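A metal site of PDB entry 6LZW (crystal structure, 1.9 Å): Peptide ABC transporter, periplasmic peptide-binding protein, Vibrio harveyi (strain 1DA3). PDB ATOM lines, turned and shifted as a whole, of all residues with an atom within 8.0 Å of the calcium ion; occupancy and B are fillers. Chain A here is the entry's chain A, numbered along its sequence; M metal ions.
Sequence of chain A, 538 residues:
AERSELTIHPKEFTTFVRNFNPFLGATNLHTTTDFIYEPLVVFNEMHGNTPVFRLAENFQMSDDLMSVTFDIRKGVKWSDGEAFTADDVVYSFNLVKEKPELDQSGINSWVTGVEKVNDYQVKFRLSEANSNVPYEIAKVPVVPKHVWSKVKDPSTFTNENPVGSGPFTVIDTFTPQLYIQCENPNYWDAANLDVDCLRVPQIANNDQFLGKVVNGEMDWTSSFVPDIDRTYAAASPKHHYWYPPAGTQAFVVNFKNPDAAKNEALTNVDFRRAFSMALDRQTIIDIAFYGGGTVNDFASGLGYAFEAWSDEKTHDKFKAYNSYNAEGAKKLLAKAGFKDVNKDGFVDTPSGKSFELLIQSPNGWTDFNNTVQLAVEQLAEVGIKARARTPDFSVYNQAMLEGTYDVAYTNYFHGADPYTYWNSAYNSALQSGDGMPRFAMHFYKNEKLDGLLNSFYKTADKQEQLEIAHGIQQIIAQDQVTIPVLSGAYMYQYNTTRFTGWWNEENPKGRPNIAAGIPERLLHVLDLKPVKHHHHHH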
ATOM      1  N   LYS A 339       6.333 -19.599  14.401  1.00  0.00           N
ATOM      2  CA  LYS A 339       5.946 -18.526  15.293  1.00  0.00           C
ATOM      3  C   LYS A 339       6.388 -17.200  14.697  1.00  0.00           C
ATOM      4  O   LYS A 339       7.495 -17.091  14.165  1.00  0.00           O
ATOM      5  CB  LYS A 339       6.589 -18.754  16.661  1.00  0.00           C
ATOM      6  CG  LYS A 339       6.347 -17.682  17.686  1.00  0.00           C
ATOM      7  CD  LYS A 339       7.098 -18.027  18.986  1.00  0.00           C
ATOM      8  CE  LYS A 339       6.912 -16.957  20.042  1.00  0.00           C
ATOM      9  NZ  LYS A 339       7.684 -17.296  21.298  1.00  0.00           N
ATOM     10  N   ASP A 340       5.528 -16.198  14.750  1.00  0.00           N
ATOM     11  CA  ASP A 340       5.947 -14.841  14.375  1.00  0.00           C
ATOM     12  C   ASP A 340       6.802 -14.244  15.501  1.00  0.00           C
ATOM     13  O   ASP A 340       6.276 -13.917  16.553  1.00  0.00           O
ATOM     14  CB  ASP A 340       4.734 -13.953  14.119  1.00  0.00           C
ATOM     15  CG  ASP A 340       5.102 -12.496  13.854  1.00  0.00           C
ATOM     16  OD1 ASP A 340       6.176 -12.240  13.254  1.00  0.00           O
ATOM     17  OD2 ASP A 340       4.326 -11.596  14.231  1.00  0.00           O
ATOM     18  N   VAL A 341       8.106 -14.092  15.287  1.00  0.00           N
ATOM     19  CA  VAL A 341       8.946 -13.495  16.327  1.00  0.00           C
ATOM     20  C   VAL A 341       9.554 -12.127  15.995  1.00  0.00           C
ATOM     21  O   VAL A 341      10.454 -11.675  16.719  1.00  0.00           O
ATOM     22  CB  VAL A 341      10.098 -14.446  16.722  1.00  0.00           C
ATOM     23  CG1 VAL A 341       9.525 -15.788  17.195  1.00  0.00           C
ATOM     24  CG2 VAL A 341      11.070 -14.641  15.547  1.00  0.00           C
ATOM     25  N   ASN A 342       9.084 -11.439  14.951  1.00  0.00           N
ATOM     26  CA  ASN A 342       9.499 -10.053  14.741  1.00  0.00           C
ATOM     27  C   ASN A 342       8.326  -9.082  14.549  1.00  0.00           C
ATOM     28  O   ASN A 342       8.475  -8.003  13.941  1.00  0.00           O
ATOM     29  CB  ASN A 342      10.471  -9.944  13.564  1.00  0.00           C
ATOM     30  CG  ASN A 342       9.811 -10.240  12.233  1.00  0.00           C
ATOM     31  OD1 ASN A 342       8.767 -10.881  12.189  1.00  0.00           O
ATOM     32  ND2 ASN A 342      10.409  -9.771  11.151  1.00  0.00           N
ATOM     33  N   LYS A 343       7.173  -9.454  15.091  1.00  0.00           N
ATOM     34  CA  LYS A 343       6.050  -8.524  15.242  1.00  0.00           C
ATOM     35  C   LYS A 343       5.509  -7.954  13.944  1.00  0.00           C
ATOM     36  O   LYS A 343       5.040  -6.826  13.937  1.00  0.00           O
ATOM     37  CB  LYS A 343       6.453  -7.331  16.139  1.00  0.00           C
ATOM     38  CG  LYS A 343       6.889  -7.694  17.546  1.00  0.00           C
ATOM     39  CD  LYS A 343       7.075  -6.447  18.405  1.00  0.00           C
ATOM     40  CE  LYS A 343       7.652  -6.820  19.759  1.00  0.00           C
ATOM     41  NZ  LYS A 343       8.985  -7.487  19.628  1.00  0.00           N
ATOM     42  N   ASP A 344       5.545  -8.714  12.848  1.00  0.00           N
ATOM     43  CA  ASP A 344       4.995  -8.184  11.598  1.00  0.00           C
ATOM     44  C   ASP A 344       3.738  -8.932  11.179  1.00  0.00           C
ATOM     45  O   ASP A 344       3.138  -8.601  10.169  1.00  0.00           O
ATOM     46  CB  ASP A 344       6.042  -8.209  10.471  1.00  0.00           C
ATOM     47  CG  ASP A 344       6.404  -9.607  10.024  1.00  0.00           C
ATOM     48  OD1 ASP A 344       6.060 -10.602  10.708  1.00  0.00           O
ATOM     49  OD2 ASP A 344       7.093  -9.709   8.993  1.00  0.00           O
ATOM     50  N   GLY A 345       3.350  -9.919  11.982  1.00  0.00           N
ATOM     51  CA  GLY A 345       2.087 -10.637  11.799  1.00  0.00           C
ATOM     52  C   GLY A 345       2.244 -11.836  10.892  1.00  0.00           C
ATOM     53  O   GLY A 345       1.276 -12.543  10.576  1.00  0.00           O
ATOM     54  N   PHE A 346       3.472 -12.062  10.452  1.00  0.00           N
ATOM     55  CA  PHE A 346       3.773 -13.147   9.527  1.00  0.00           C
ATOM     56  C   PHE A 346       4.672 -14.176  10.205  1.00  0.00           C
ATOM     57  O   PHE A 346       5.741 -13.848  10.727  1.00  0.00           O
ATOM     58  CB  PHE A 346       4.417 -12.577   8.240  1.00  0.00           C
ATOM     59  CG  PHE A 346       3.445 -11.803   7.371  1.00  0.00           C
ATOM     60  CD1 PHE A 346       2.466 -12.469   6.641  1.00  0.00           C
ATOM     61  CD2 PHE A 346       3.512 -10.420   7.275  1.00  0.00           C
ATOM     62  CE1 PHE A 346       1.562 -11.756   5.825  1.00  0.00           C
ATOM     63  CE2 PHE A 346       2.617  -9.719   6.474  1.00  0.00           C
ATOM     64  CZ  PHE A 346       1.655 -10.378   5.753  1.00  0.00           C
ATOM     65  N   VAL A 347       4.239 -15.443  10.203  1.00  0.00           N
ATOM     66  CA  VAL A 347       4.964 -16.484  10.923  1.00  0.00           C
ATOM     67  C   VAL A 347       6.355 -16.623  10.338  1.00  0.00           C
ATOM     68  O   VAL A 347       6.549 -16.456   9.135  1.00  0.00           O
ATOM     69  CB  VAL A 347       4.244 -17.874  10.876  1.00  0.00           C
ATOM     70  CG1 VAL A 347       2.778 -17.740  11.245  1.00  0.00           C
ATOM     71  CG2 VAL A 347       4.416 -18.525   9.511  1.00  0.00           C
ATOM     72  N   ASP A 348       7.324 -16.900  11.203  1.00  0.00           N
ATOM     73  CA  ASP A 348       8.685 -17.152  10.756  1.00  0.00           C
ATOM     74  C   ASP A 348       9.029 -18.632  10.944  1.00  0.00           C
ATOM     75  O   ASP A 348       8.289 -19.359  11.607  1.00  0.00           O
ATOM     76  CB  ASP A 348       9.647 -16.226  11.528  1.00  0.00           C
ATOM     77  CG  ASP A 348       9.143 -14.783  11.556  1.00  0.00           C
ATOM     78  OD1 ASP A 348       9.047 -14.156  10.462  1.00  0.00           O
ATOM     79  OD2 ASP A 348       8.855 -14.252  12.663  1.00  0.00           O
ATOM     80  N   THR A 349      10.100 -19.098  10.322  1.00  0.00           N
ATOM     81  CA  THR A 349      10.492 -20.510  10.415  1.00  0.00           C
ATOM     82  C   THR A 349      10.857 -20.924  11.857  1.00  0.00           C
ATOM     83  O   THR A 349      11.077 -20.074  12.722  1.00  0.00           O
ATOM     84  CB  THR A 349      11.698 -20.817   9.490  1.00  0.00           C
ATOM     85  OG1 THR A 349      12.884 -20.189  10.020  1.00  0.00           O
ATOM     86  CG2 THR A 349      11.446 -20.332   8.076  1.00  0.00           C
ATOM     87  N   GLY A 352      13.707 -19.376  13.264  1.00  0.00           N
ATOM     88  CA  GLY A 352      13.510 -17.953  13.496  1.00  0.00           C
ATOM     89  C   GLY A 352      13.698 -17.051  12.298  1.00  0.00           C
ATOM     90  O   GLY A 352      13.820 -15.836  12.447  1.00  0.00           O
ATOM     91  N   LYS A 353      13.699 -17.616  11.100  1.00  0.00           N
ATOM     92  CA  LYS A 353      13.898 -16.780   9.928  1.00  0.00           C
ATOM     93  C   LYS A 353      12.588 -16.314   9.314  1.00  0.00           C
ATOM     94  O   LYS A 353      11.639 -17.088   9.146  1.00  0.00           O
ATOM     95  CB  LYS A 353      14.731 -17.531   8.887  1.00  0.00           C
ATOM     96  CG  LYS A 353      16.024 -18.111   9.462  1.00  0.00           C
ATOM     97  CD  LYS A 353      16.728 -18.964   8.400  1.00  0.00           C
ATOM     98  CE  LYS A 353      18.195 -19.179   8.739  1.00  0.00           C
ATOM     99  NZ  LYS A 353      18.417 -20.376   9.638  1.00  0.00           N
ATOM    100  N   SER A 354      12.546 -15.015   9.013  1.00  0.00           N
ATOM    101  CA  SER A 354      11.480 -14.400   8.235  1.00  0.00           C
ATOM    102  C   SER A 354      11.536 -14.872   6.799  1.00  0.00           C
ATOM    103  O   SER A 354      12.627 -15.143   6.265  1.00  0.00           O
ATOM    104  CB  SER A 354      11.597 -12.869   8.296  1.00  0.00           C
ATOM    105  OG  SER A 354      11.154 -12.397   9.535  1.00  0.00           O
ATOM    106  N   PHE A 355      10.387 -14.976   6.148  1.00  0.00           N
ATOM    107  CA  PHE A 355      10.384 -15.319   4.725  1.00  0.00           C
ATOM    108  C   PHE A 355       9.123 -14.886   3.955  1.00  0.00           C
ATOM    109  O   PHE A 355       8.054 -14.601   4.527  1.00  0.00           O
ATOM    110  CB  PHE A 355      10.633 -16.832   4.554  1.00  0.00           C
ATOM    111  CG  PHE A 355       9.511 -17.715   5.059  1.00  0.00           C
ATOM    112  CD1 PHE A 355       9.421 -18.036   6.406  1.00  0.00           C
ATOM    113  CD2 PHE A 355       8.575 -18.254   4.177  1.00  0.00           C
ATOM    114  CE1 PHE A 355       8.400 -18.855   6.877  1.00  0.00           C
ATOM    115  CE2 PHE A 355       7.559 -19.077   4.641  1.00  0.00           C
ATOM    116  CZ  PHE A 355       7.472 -19.374   5.988  1.00  0.00           C
ATOM    117  N   GLY A 383      -1.447 -15.676   8.267  1.00  0.00           N
ATOM    118  CA  GLY A 383      -0.112 -15.193   8.581  1.00  0.00           C
ATOM    119  C   GLY A 383       1.019 -15.825   7.770  1.00  0.00           C
ATOM    120  O   GLY A 383       2.172 -15.809   8.208  1.00  0.00           O
ATOM    121  N   LYS A 385       3.274 -15.271   4.542  1.00  0.00           N
ATOM    122  CA  LYS A 385       3.611 -14.165   3.632  1.00  0.00           C
ATOM    123  C   LYS A 385       4.006 -14.661   2.255  1.00  0.00           C
ATOM    124  O   LYS A 385       4.925 -15.472   2.106  1.00  0.00           O
ATOM    125  CB  LYS A 385       4.743 -13.293   4.216  1.00  0.00           C
ATOM    126  CG  LYS A 385       4.887 -11.918   3.578  1.00  0.00           C
ATOM    127  CD  LYS A 385       5.809 -11.041   4.438  1.00  0.00           C
ATOM    128  CE  LYS A 385       6.103  -9.685   3.803  1.00  0.00           C
ATOM    129  NZ  LYS A 385       7.253  -8.979   4.498  1.00  0.00           N
HETATM  130 CA    CA M   1       7.506 -12.619  11.346  1.00  0.00          CA
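O of Phe 346 binds the calcium ion (2.2 Å).
The calcium ion is bound by OD1 of Asn 342.
OD1 of Asp 348 binds the calcium ion, at 2.3 Å.
OD1 of Asp 340 is bound to the calcium ion (2.4 Å).
The calcium ion is bound by the side-chain carboxylate (OD2) of Asp 348 (2.5 Å).
The calcium ion is bound by OD1 of Asp 344, at 2.6 Å.
The nearest printed residue that does not touch the calcium ion is Ser 354 (4.1 Å).
N of Asp 348 is in hydrogen-bond range of O of Lys 339 (3.0 Å).
OG of Ser 354 sits close to OD1 of Asp 348.
The side-chain carboxylate of Asp 348 lies close to the backbone NH of Val 341 (2.7 Å).
The side-chain carboxylate (OD1) of Asp 340 lies close to the backbone NH (N) of Lys 343 (3.5 Å).
The side-chain carboxylate of Asp 340 sits at hydrogen-bond distance from the backbone NH of Gly 345.
The side-chain hydroxyl of Ser 354 sits at hydrogen-bond distance from the side-chain amide nitrogen of Asn 342 (3.2 Å).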
